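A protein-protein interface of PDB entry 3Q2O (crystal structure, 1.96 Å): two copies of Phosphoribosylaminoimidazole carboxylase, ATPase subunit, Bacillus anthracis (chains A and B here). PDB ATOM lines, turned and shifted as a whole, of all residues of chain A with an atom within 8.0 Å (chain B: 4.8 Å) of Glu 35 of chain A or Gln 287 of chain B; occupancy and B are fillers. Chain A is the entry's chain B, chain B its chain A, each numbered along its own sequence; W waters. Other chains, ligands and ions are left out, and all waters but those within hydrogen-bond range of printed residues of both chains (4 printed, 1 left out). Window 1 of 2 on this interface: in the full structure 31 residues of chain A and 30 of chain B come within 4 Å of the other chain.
NE2 of Gln 287 of chain B is in hydrogen-bond range of OE1 of Glu 35 of chain A (3.2 Å).
A ring nitrogen (ND1) of His 342 of chain B lies within hydrogen-bond range of the side-chain carboxylate of Glu 35 of chain A, at 3.0 Å.
N of Leu 343 of chain B sits at hydrogen-bond distance from O of Glu 35 of chain A (2.9 Å).
O of Leu 343 of chain B lies close to N of Gly 37 of chain A, at 3.5 Å.
SD of Met 28 of chain B sits at hydrogen-bond distance from NE2 of Gln 287 of chain B (3.5 Å).
ND1 of His 342 of chain B lies within hydrogen-bond range of OE1 of Gln 287 of chain B, 3.2 Å away.
The side-chain amide oxygen (OE1) of Gln 287 of chain B lies within hydrogen-bond range of a ring nitrogen (NE2) of His 357 of chain B, 2.7 Å away.
NE2 of His 342 of chain B sits at hydrogen-bond distance from OD2 of Asp 288 of chain B, at 2.7 Å.
The backbone carbonyl oxygen (O) of His 342 of chain B lies within hydrogen-bond range of the backbone NH (N) of His 357 of chain B, at 2.8 Å.
NH1 of Arg 300 of chain A sits at hydrogen-bond distance from SD of Met 36 of chain A, 3.7 Å away.
Among the printed residues, pairs that only touch across the chains: Pro 13 of chain A with Leu 341 of chain B, Pro 13 of chain A with Leu 343 of chain B, Leu 31 of chain A with Leu 31 of chain B, Lys 34 of chain A with Leu 31 of chain B, Lys 34 of chain A with Leu 343 of chain B, Glu 35 of chain A with Leu 31 of chain B, Met 36 of chain A with Leu 341 of chain B and Met 36 of chain A with Leu 343 of chain B.
Of the printed residues of chain B, Glu 35 of chain A touches Leu 31, Gln 287, His 342 and Leu 343.
Gln 287 of chain B touches one residue of chain A.
Printed residues of chain B within 4 Å of Pro 13 of chain A: Leu 341 (3.97 Å) and Leu 343 (3.5 Å).
Printed residues of chain B within 4 Å of Met 36 of chain A: Leu 341 and Leu 343.
Printed residues of chain A within 4 Å of Leu 31 of chain B: Leu 31, Lys 34 and Glu 35.
The nearest printed residue of chain B that does not touch Glu 35 of chain A is Leu 341 of chain B (4.02 Å).
Printed residues of chain B that touch a printed residue of chain A: Leu 31, Gln 287, Leu 341, His 342 and Leu 343.
Of the 17 printed residues of chain A, 6 touch a printed residue of chain B.
Printed residues of chain A that touch a printed residue of chain B: Pro 13, Leu 31, Lys 34, Glu 35, Met 36 and Gly 37.
Among the printed residues, 12 pairs touch across the chains.
Leu 31 of chain A touches its own counterpart, Leu 31 of chain B.
2 positions are printed for both chains.
Water W4 lies within hydrogen-bond range of the backbone carbonyl oxygen (O) of Met 28 of chain B (2.6 Å), the side-chain carboxylate (OE2) of Glu 35 of chain A (3.1 Å) and the side-chain amide nitrogen (NE2) of Gln 287 of chain B (3.5 Å).
Water W3 lies within hydrogen-bond range of the backbone carbonyl oxygen (O) of Glu 291 of chain A (2.7 Å) and the side-chain carboxylate (OD1) of Asp 288 of chain B (3.0 Å).
Water W2 lies within hydrogen-bond range of O of Leu 341 of chain B (2.8 Å) and NH2 of Arg 300 of chain A (3.0 Å).
Water W1 lies within hydrogen-bond range of the backbone NH (N) of Leu 341 of chain B (3.3 Å) and the guanidinium group (NH2) of Arg 300 of chain A (3.4 Å).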
ATOM      1  N   PRO A  13      31.693   7.654 -20.507  1.00  0.00           N
ATOM      2  CA  PRO A  13      31.420   9.084 -20.432  1.00  0.00           C
ATOM      3  C   PRO A  13      32.587   9.873 -21.016  1.00  0.00           C
ATOM      4  O   PRO A  13      33.737   9.452 -20.874  1.00  0.00           O
ATOM      5  CB  PRO A  13      31.314   9.326 -18.930  1.00  0.00           C
ATOM      6  CG  PRO A  13      30.710   8.094 -18.420  1.00  0.00           C
ATOM      7  CD  PRO A  13      31.342   6.975 -19.245  1.00  0.00           C
ATOM      8  N   MET A  29      16.964  12.305 -24.823  1.00  0.00           N
ATOM      9  CA  MET A  29      18.142  11.416 -24.804  1.00  0.00           C
ATOM     10  C   MET A  29      19.399  12.231 -24.535  1.00  0.00           C
ATOM     11  O   MET A  29      20.263  11.825 -23.743  1.00  0.00           O
ATOM     12  CB  MET A  29      18.346  10.709 -26.154  1.00  0.00           C
ATOM     13  CG  MET A  29      17.499   9.476 -26.400  1.00  0.00           C
ATOM     14  SD  MET A  29      17.886   8.857 -28.056  1.00  0.00           S
ATOM     15  CE  MET A  29      16.543   7.684 -28.306  1.00  0.00           C
ATOM     16  N   ALA A  30      19.500  13.369 -25.226  1.00  0.00           N
ATOM     17  CA  ALA A  30      20.697  14.210 -25.164  1.00  0.00           C
ATOM     18  C   ALA A  30      20.894  14.812 -23.776  1.00  0.00           C
ATOM     19  O   ALA A  30      21.998  14.805 -23.242  1.00  0.00           O
ATOM     20  CB  ALA A  30      20.634  15.303 -26.215  1.00  0.00           C
ATOM     21  N   LEU A  31      19.823  15.346 -23.200  1.00  0.00           N
ATOM     22  CA  LEU A  31      19.900  15.927 -21.864  1.00  0.00           C
ATOM     23  C   LEU A  31      20.352  14.912 -20.814  1.00  0.00           C
ATOM     24  O   LEU A  31      21.180  15.219 -19.965  1.00  0.00           O
ATOM     25  CB  LEU A  31      18.564  16.568 -21.480  1.00  0.00           C
ATOM     26  CG  LEU A  31      18.231  17.841 -22.265  1.00  0.00           C
ATOM     27  CD1 LEU A  31      16.753  18.176 -22.149  1.00  0.00           C
ATOM     28  CD2 LEU A  31      19.094  19.011 -21.784  1.00  0.00           C
ATOM     29  N   ALA A  32      19.826  13.695 -20.898  1.00  0.00           N
ATOM     30  CA  ALA A  32      20.222  12.610 -20.005  1.00  0.00           C
ATOM     31  C   ALA A  32      21.694  12.262 -20.198  1.00  0.00           C
ATOM     32  O   ALA A  32      22.422  12.101 -19.218  1.00  0.00           O
ATOM     33  CB  ALA A  32      19.332  11.366 -20.232  1.00  0.00           C
ATOM     34  N   ALA A  33      22.131  12.161 -21.457  1.00  0.00           N
ATOM     35  CA  ALA A  33      23.530  11.854 -21.768  1.00  0.00           C
ATOM     36  C   ALA A  33      24.487  12.953 -21.287  1.00  0.00           C
ATOM     37  O   ALA A  33      25.600  12.661 -20.856  1.00  0.00           O
ATOM     38  CB  ALA A  33      23.717  11.603 -23.276  1.00  0.00           C
ATOM     39  N   LYS A  34      24.046  14.208 -21.361  1.00  0.00           N
ATOM     40  CA  LYS A  34      24.853  15.356 -20.908  1.00  0.00           C
ATOM     41  C   LYS A  34      25.126  15.332 -19.405  1.00  0.00           C
ATOM     42  O   LYS A  34      26.211  15.742 -18.962  1.00  0.00           O
ATOM     43  CB  LYS A  34      24.182  16.680 -21.280  1.00  0.00           C
ATOM     44  CG  LYS A  34      24.246  17.028 -22.751  1.00  0.00           C
ATOM     45  CD  LYS A  34      25.606  17.559 -23.115  1.00  0.00           C
ATOM     46  CE  LYS A  34      25.548  18.374 -24.392  1.00  0.00           C
ATOM     47  NZ  LYS A  34      26.889  18.960 -24.666  1.00  0.00           N
ATOM     48  N   GLU A  35      24.148  14.867 -18.621  1.00  0.00           N
ATOM     49  CA  GLU A  35      24.328  14.748 -17.173  1.00  0.00           C
ATOM     50  C   GLU A  35      25.499  13.823 -16.860  1.00  0.00           C
ATOM     51  O   GLU A  35      26.256  14.081 -15.926  1.00  0.00           O
ATOM     52  CB  GLU A  35      23.057  14.246 -16.470  1.00  0.00           C
ATOM     53  CG  GLU A  35      21.928  15.283 -16.347  1.00  0.00           C
ATOM     54  CD  GLU A  35      22.121  16.315 -15.230  1.00  0.00           C
ATOM     55  OE1 GLU A  35      23.159  16.304 -14.494  1.00  0.00           O
ATOM     56  OE2 GLU A  35      21.215  17.175 -15.095  1.00  0.00           O
ATOM     57  N   MET A  36      25.646  12.770 -17.668  1.00  0.00           N
ATOM     58  CA  MET A  36      26.707  11.783 -17.496  1.00  0.00           C
ATOM     59  C   MET A  36      28.028  12.174 -18.162  1.00  0.00           C
ATOM     60  O   MET A  36      28.997  11.430 -18.067  1.00  0.00           O
ATOM     61  CB  MET A  36      26.248  10.402 -18.001  1.00  0.00           C
ATOM     62  CG  MET A  36      25.051   9.872 -17.250  1.00  0.00           C
ATOM     63  SD  MET A  36      24.680   8.146 -17.591  1.00  0.00           S
ATOM     64  CE  MET A  36      25.948   7.371 -16.594  1.00  0.00           C
ATOM     65  N   GLY A  37      28.069  13.323 -18.840  1.00  0.00           N
ATOM     66  CA  GLY A  37      29.314  13.821 -19.430  1.00  0.00           C
ATOM     67  C   GLY A  37      29.618  13.382 -20.859  1.00  0.00           C
ATOM     68  O   GLY A  37      30.765  13.486 -21.319  1.00  0.00           O
ATOM     69  N   TYR A  38      28.597  12.893 -21.564  1.00  0.00           N
ATOM     70  CA  TYR A  38      28.731  12.566 -22.986  1.00  0.00           C
ATOM     71  C   TYR A  38      28.601  13.810 -23.849  1.00  0.00           C
ATOM     72  O   TYR A  38      27.888  14.744 -23.492  1.00  0.00           O
ATOM     73  CB  TYR A  38      27.665  11.554 -23.420  1.00  0.00           C
ATOM     74  CG  TYR A  38      27.897  10.182 -22.847  1.00  0.00           C
ATOM     75  CD1 TYR A  38      28.793   9.293 -23.457  1.00  0.00           C
ATOM     76  CD2 TYR A  38      27.237   9.771 -21.686  1.00  0.00           C
ATOM     77  CE1 TYR A  38      29.022   8.024 -22.921  1.00  0.00           C
ATOM     78  CE2 TYR A  38      27.462   8.505 -21.136  1.00  0.00           C
ATOM     79  CZ  TYR A  38      28.358   7.639 -21.756  1.00  0.00           C
ATOM     80  OH  TYR A  38      28.576   6.381 -21.223  1.00  0.00           O
ATOM     81  N   ILE A  40      27.289  15.119 -27.669  1.00  0.00           N
ATOM     82  CA  ILE A  40      26.156  14.738 -28.519  1.00  0.00           C
ATOM     83  C   ILE A  40      26.256  15.328 -29.919  1.00  0.00           C
ATOM     84  O   ILE A  40      26.439  16.546 -30.095  1.00  0.00           O
ATOM     85  CB  ILE A  40      24.780  15.168 -27.913  1.00  0.00           C
ATOM     86  CG1 ILE A  40      24.508  14.487 -26.560  1.00  0.00           C
ATOM     87  CG2 ILE A  40      23.643  14.912 -28.914  1.00  0.00           C
ATOM     88  CD1 ILE A  40      24.168  12.979 -26.617  1.00  0.00           C
ATOM     89  N   VAL A  54      20.497  21.191 -27.797  1.00  0.00           N
ATOM     90  CA  VAL A  54      21.249  20.607 -26.678  1.00  0.00           C
ATOM     91  C   VAL A  54      22.530  19.884 -27.137  1.00  0.00           C
ATOM     92  O   VAL A  54      23.399  19.567 -26.330  1.00  0.00           O
ATOM     93  CB  VAL A  54      20.341  19.685 -25.788  1.00  0.00           C
ATOM     94  CG1 VAL A  54      19.555  18.706 -26.624  1.00  0.00           C
ATOM     95  CG2 VAL A  54      21.157  18.933 -24.744  1.00  0.00           C
ATOM     96  N   GLN A 287      10.627  10.476 -16.214  1.00  0.00           N
ATOM     97  CA  GLN A 287      11.567  11.586 -15.941  1.00  0.00           C
ATOM     98  C   GLN A 287      11.422  12.130 -14.525  1.00  0.00           C
ATOM     99  O   GLN A 287      12.381  12.625 -13.961  1.00  0.00           O
ATOM    100  CB  GLN A 287      11.354  12.751 -16.897  1.00  0.00           C
ATOM    101  CG  GLN A 287      11.712  12.463 -18.339  1.00  0.00           C
ATOM    102  CD  GLN A 287      11.558  13.701 -19.193  1.00  0.00           C
ATOM    103  OE1 GLN A 287      10.463  14.252 -19.317  1.00  0.00           O
ATOM    104  NE2 GLN A 287      12.659  14.164 -19.762  1.00  0.00           N
ATOM    105  N   CYS A 290      10.332   7.970 -11.635  1.00  0.00           N
ATOM    106  CA  CYS A 290      11.170   6.775 -11.461  1.00  0.00           C
ATOM    107  C   CYS A 290      12.590   7.130 -11.089  1.00  0.00           C
ATOM    108  O   CYS A 290      13.029   8.260 -11.276  1.00  0.00           O
ATOM    109  CB  CYS A 290      11.180   5.908 -12.728  1.00  0.00           C
ATOM    110  SG  CYS A 290       9.589   5.144 -13.056  1.00  0.00           S
ATOM    111  N   GLU A 291      13.301   6.141 -10.570  1.00  0.00           N
ATOM    112  CA  GLU A 291      14.673   6.312 -10.139  1.00  0.00           C
ATOM    113  C   GLU A 291      15.575   6.621 -11.351  1.00  0.00           C
ATOM    114  O   GLU A 291      16.532   7.380 -11.233  1.00  0.00           O
ATOM    115  CB  GLU A 291      15.106   5.047  -9.395  1.00  0.00           C
ATOM    116  CG  GLU A 291      16.258   5.203  -8.428  1.00  0.00           C
ATOM    117  CD  GLU A 291      16.498   3.936  -7.604  1.00  0.00           C
ATOM    118  OE1 GLU A 291      17.677   3.501  -7.486  1.00  0.00           O
ATOM    119  OE2 GLU A 291      15.497   3.373  -7.088  1.00  0.00           O
ATOM    120  N   ARG A 300      22.313   4.406 -21.108  1.00  0.00           N
ATOM    121  CA  ARG A 300      23.038   3.354 -20.405  1.00  0.00           C
ATOM    122  C   ARG A 300      23.038   2.054 -21.214  1.00  0.00           C
ATOM    123  O   ARG A 300      24.057   1.358 -21.266  1.00  0.00           O
ATOM    124  CB  ARG A 300      22.438   3.096 -19.018  1.00  0.00           C
ATOM    125  CG  ARG A 300      22.750   4.162 -17.971  1.00  0.00           C
ATOM    126  CD  ARG A 300      21.781   4.076 -16.793  1.00  0.00           C
ATOM    127  NE  ARG A 300      22.145   5.011 -15.717  1.00  0.00           N
ATOM    128  CZ  ARG A 300      21.908   6.325 -15.735  1.00  0.00           C
ATOM    129  NH1 ARG A 300      21.301   6.890 -16.773  1.00  0.00           N
ATOM    130  NH2 ARG A 300      22.280   7.083 -14.704  1.00  0.00           N
ATOM    131  N   MET B  28      24.469  22.567 -14.534  1.00  0.00           N
ATOM    132  CA  MET B  28      23.298  21.882 -13.993  1.00  0.00           C
ATOM    133  C   MET B  28      22.040  22.763 -13.921  1.00  0.00           C
ATOM    134  O   MET B  28      20.914  22.250 -14.049  1.00  0.00           O
ATOM    135  CB  MET B  28      23.636  21.236 -12.652  1.00  0.00           C
ATOM    136  CG  MET B  28      24.471  19.966 -12.826  1.00  0.00           C
ATOM    137  SD  MET B  28      25.022  19.206 -11.291  1.00  0.00           S
ATOM    138  CE  MET B  28      26.354  20.255 -10.733  1.00  0.00           C
ATOM    139  N   LEU B  31      20.847  22.724 -17.620  1.00  0.00           N
ATOM    140  CA  LEU B  31      20.189  21.461 -17.963  1.00  0.00           C
ATOM    141  C   LEU B  31      18.763  21.392 -17.428  1.00  0.00           C
ATOM    142  O   LEU B  31      17.856  20.954 -18.132  1.00  0.00           O
ATOM    143  CB  LEU B  31      21.004  20.265 -17.470  1.00  0.00           C
ATOM    144  CG  LEU B  31      22.332  20.049 -18.211  1.00  0.00           C
ATOM    145  CD1 LEU B  31      23.255  19.191 -17.368  1.00  0.00           C
ATOM    146  CD2 LEU B  31      22.109  19.414 -19.581  1.00  0.00           C
ATOM    147  N   GLY B 283      23.901  19.978  -2.026  1.00  0.00           N
ATOM    148  CA  GLY B 283      22.552  19.749  -2.538  1.00  0.00           C
ATOM    149  C   GLY B 283      22.467  18.921  -3.811  1.00  0.00           C
ATOM    150  O   GLY B 283      21.380  18.778  -4.379  1.00  0.00           O
ATOM    151  N   HIS B 284      23.593  18.393  -4.293  1.00  0.00           N
ATOM    152  CA  HIS B 284      23.575  17.621  -5.557  1.00  0.00           C
ATOM    153  C   HIS B 284      22.750  16.338  -5.444  1.00  0.00           C
ATOM    154  O   HIS B 284      22.204  15.840  -6.440  1.00  0.00           O
ATOM    155  CB  HIS B 284      24.993  17.283  -6.051  1.00  0.00           C
ATOM    156  CG  HIS B 284      25.796  18.478  -6.476  1.00  0.00           C
ATOM    157  ND1 HIS B 284      25.231  19.709  -6.727  1.00  0.00           N
ATOM    158  CD2 HIS B 284      27.120  18.616  -6.728  1.00  0.00           C
ATOM    159  CE1 HIS B 284      26.171  20.561  -7.092  1.00  0.00           C
ATOM    160  NE2 HIS B 284      27.328  19.924  -7.099  1.00  0.00           N
ATOM    161  N   TYR B 285      22.655  15.812  -4.225  1.00  0.00           N
ATOM    162  CA  TYR B 285      21.819  14.625  -3.958  1.00  0.00           C
ATOM    163  C   TYR B 285      20.392  14.777  -4.488  1.00  0.00           C
ATOM    164  O   TYR B 285      19.742  13.775  -4.830  1.00  0.00           O
ATOM    165  CB  TYR B 285      21.767  14.331  -2.457  1.00  0.00           C
ATOM    166  CG  TYR B 285      20.866  15.252  -1.641  1.00  0.00           C
ATOM    167  CD1 TYR B 285      21.372  16.393  -1.016  1.00  0.00           C
ATOM    168  CD2 TYR B 285      19.516  14.951  -1.470  1.00  0.00           C
ATOM    169  CE1 TYR B 285      20.536  17.226  -0.241  1.00  0.00           C
ATOM    170  CE2 TYR B 285      18.678  15.766  -0.717  1.00  0.00           C
ATOM    171  CZ  TYR B 285      19.189  16.896  -0.107  1.00  0.00           C
ATOM    172  OH  TYR B 285      18.328  17.670   0.631  1.00  0.00           O
ATOM    173  N   THR B 286      19.911  16.027  -4.528  1.00  0.00           N
ATOM    174  CA  THR B 286      18.528  16.332  -4.913  1.00  0.00           C
ATOM    175  C   THR B 286      18.216  15.962  -6.355  1.00  0.00           C
ATOM    176  O   THR B 286      17.048  15.768  -6.704  1.00  0.00           O
ATOM    177  CB  THR B 286      18.176  17.840  -4.749  1.00  0.00           C
ATOM    178  OG1 THR B 286      19.060  18.626  -5.565  1.00  0.00           O
ATOM    179  CG2 THR B 286      18.292  18.270  -3.278  1.00  0.00           C
ATOM    180  N   GLN B 287      19.247  15.884  -7.188  1.00  0.00           N
ATOM    181  CA  GLN B 287      19.071  15.534  -8.587  1.00  0.00           C
ATOM    182  C   GLN B 287      18.440  14.156  -8.764  1.00  0.00           C
ATOM    183  O   GLN B 287      17.673  13.953  -9.689  1.00  0.00           O
ATOM    184  CB  GLN B 287      20.408  15.528  -9.309  1.00  0.00           C
ATOM    185  CG  GLN B 287      21.020  16.897  -9.535  1.00  0.00           C
ATOM    186  CD  GLN B 287      22.198  16.778 -10.451  1.00  0.00           C
ATOM    187  OE1 GLN B 287      23.200  16.131 -10.117  1.00  0.00           O
ATOM    188  NE2 GLN B 287      22.075  17.349 -11.638  1.00  0.00           N
ATOM    189  N   ASP B 288      18.774  13.218  -7.885  1.00  0.00           N
ATOM    190  CA  ASP B 288      18.286  11.847  -8.054  1.00  0.00           C
ATOM    191  C   ASP B 288      17.363  11.372  -6.946  1.00  0.00           C
ATOM    192  O   ASP B 288      16.617  10.416  -7.134  1.00  0.00           O
ATOM    193  CB  ASP B 288      19.464  10.891  -8.242  1.00  0.00           C
ATOM    194  CG  ASP B 288      20.242  11.188  -9.512  1.00  0.00           C
ATOM    195  OD1 ASP B 288      19.652  11.078 -10.612  1.00  0.00           O
ATOM    196  OD2 ASP B 288      21.426  11.550  -9.411  1.00  0.00           O
ATOM    197  N   ALA B 289      17.394  12.055  -5.800  1.00  0.00           N
ATOM    198  CA  ALA B 289      16.679  11.560  -4.626  1.00  0.00           C
ATOM    199  C   ALA B 289      15.433  12.360  -4.236  1.00  0.00           C
ATOM    200  O   ALA B 289      14.649  11.903  -3.399  1.00  0.00           O
ATOM    201  CB  ALA B 289      17.626  11.452  -3.441  1.00  0.00           C
ATOM    202  N   SER B 293      14.944  18.909  -8.171  1.00  0.00           N
ATOM    203  CA  SER B 293      16.335  19.170  -7.821  1.00  0.00           C
ATOM    204  C   SER B 293      16.522  20.622  -7.406  1.00  0.00           C
ATOM    205  O   SER B 293      15.706  21.479  -7.745  1.00  0.00           O
ATOM    206  CB  SER B 293      17.279  18.823  -8.981  1.00  0.00           C
ATOM    207  OG  SER B 293      17.381  19.904  -9.892  1.00  0.00           O
ATOM    208  N   PHE B 295      18.431  22.561  -8.683  1.00  0.00           N
ATOM    209  CA  PHE B 295      18.593  23.315  -9.923  1.00  0.00           C
ATOM    210  C   PHE B 295      17.262  23.651 -10.569  1.00  0.00           C
ATOM    211  O   PHE B 295      17.045  24.800 -10.997  1.00  0.00           O
ATOM    212  CB  PHE B 295      19.529  22.573 -10.894  1.00  0.00           C
ATOM    213  CG  PHE B 295      20.872  22.283 -10.301  1.00  0.00           C
ATOM    214  CD1 PHE B 295      21.174  21.014  -9.832  1.00  0.00           C
ATOM    215  CD2 PHE B 295      21.815  23.307 -10.162  1.00  0.00           C
ATOM    216  CE1 PHE B 295      22.417  20.750  -9.246  1.00  0.00           C
ATOM    217  CE2 PHE B 295      23.048  23.068  -9.574  1.00  0.00           C
ATOM    218  CZ  PHE B 295      23.359  21.775  -9.116  1.00  0.00           C
ATOM    219  N   LEU B 341      25.530   8.574 -11.932  1.00  0.00           N
ATOM    220  CA  LEU B 341      26.751   9.292 -12.245  1.00  0.00           C
ATOM    221  C   LEU B 341      26.467  10.624 -12.913  1.00  0.00           C
ATOM    222  O   LEU B 341      25.643  10.712 -13.825  1.00  0.00           O
ATOM    223  CB  LEU B 341      27.656   8.418 -13.132  1.00  0.00           C
ATOM    224  CG  LEU B 341      28.982   8.973 -13.643  1.00  0.00           C
ATOM    225  CD1 LEU B 341      29.875   9.373 -12.467  1.00  0.00           C
ATOM    226  CD2 LEU B 341      29.702   7.968 -14.577  1.00  0.00           C
ATOM    227  N   HIS B 342      27.151  11.661 -12.436  1.00  0.00           N
ATOM    228  CA  HIS B 342      27.089  12.982 -13.032  1.00  0.00           C
ATOM    229  C   HIS B 342      28.517  13.448 -13.294  1.00  0.00           C
ATOM    230  O   HIS B 342      29.328  13.505 -12.366  1.00  0.00           O
ATOM    231  CB  HIS B 342      26.373  13.954 -12.087  1.00  0.00           C
ATOM    232  CG  HIS B 342      24.939  13.607 -11.844  1.00  0.00           C
ATOM    233  ND1 HIS B 342      23.911  14.173 -12.564  1.00  0.00           N
ATOM    234  CD2 HIS B 342      24.361  12.724 -10.994  1.00  0.00           C
ATOM    235  CE1 HIS B 342      22.759  13.671 -12.154  1.00  0.00           C
ATOM    236  NE2 HIS B 342      23.005  12.784 -11.209  1.00  0.00           N
ATOM    237  N   LEU B 343      28.826  13.759 -14.549  1.00  0.00           N
ATOM    238  CA  LEU B 343      30.150  14.283 -14.911  1.00  0.00           C
ATOM    239  C   LEU B 343      30.004  15.590 -15.682  1.00  0.00           C
ATOM    240  O   LEU B 343      29.145  15.722 -16.549  1.00  0.00           O
ATOM    241  CB  LEU B 343      30.970  13.249 -15.700  1.00  0.00           C
ATOM    242  CG  LEU B 343      31.361  11.982 -14.912  1.00  0.00           C
ATOM    243  CD1 LEU B 343      31.906  10.874 -15.843  1.00  0.00           C
ATOM    244  CD2 LEU B 343      32.381  12.282 -13.811  1.00  0.00           C
ATOM    245  N   HIS B 357      29.980  14.034  -9.690  1.00  0.00           N
ATOM    246  CA  HIS B 357      29.538  13.407  -8.440  1.00  0.00           C
ATOM    247  C   HIS B 357      28.747  12.142  -8.735  1.00  0.00           C
ATOM    248  O   HIS B 357      28.259  11.955  -9.848  1.00  0.00           O
ATOM    249  CB  HIS B 357      28.724  14.384  -7.558  1.00  0.00           C
ATOM    250  CG  HIS B 357      27.416  14.810  -8.159  1.00  0.00           C
ATOM    251  ND1 HIS B 357      27.314  15.885  -9.016  1.00  0.00           N
ATOM    252  CD2 HIS B 357      26.164  14.303  -8.037  1.00  0.00           C
ATOM    253  CE1 HIS B 357      26.054  16.028  -9.390  1.00  0.00           C
ATOM    254  NE2 HIS B 357      25.340  15.067  -8.831  1.00  0.00           N
ATOM    255  N   ASN B 359      25.486   9.947  -7.095  1.00  0.00           N
ATOM    256  CA  ASN B 359      24.420   9.763  -6.120  1.00  0.00           C
ATOM    257  C   ASN B 359      24.091   8.290  -5.981  1.00  0.00           C
ATOM    258  O   ASN B 359      23.625   7.653  -6.946  1.00  0.00           O
ATOM    259  CB  ASN B 359      23.171  10.553  -6.548  1.00  0.00           C
ATOM    260  CG  ASN B 359      23.341  12.050  -6.363  1.00  0.00           C
ATOM    261  OD1 ASN B 359      24.090  12.491  -5.485  1.00  0.00           O
ATOM    262  ND2 ASN B 359      22.649  12.838  -7.177  1.00  0.00           N
HETATM  263  O   HOH W   1      25.156   5.708 -13.499  1.00  0.00           O
HETATM  264  O   HOH W   2      22.952   9.999 -14.185  1.00  0.00           O
HETATM  265  O   HOH W   3      18.252   9.129 -12.378  1.00  0.00           O
HETATM  266  O   HOH W   4      20.375  19.714 -13.548  1.00  0.00           O
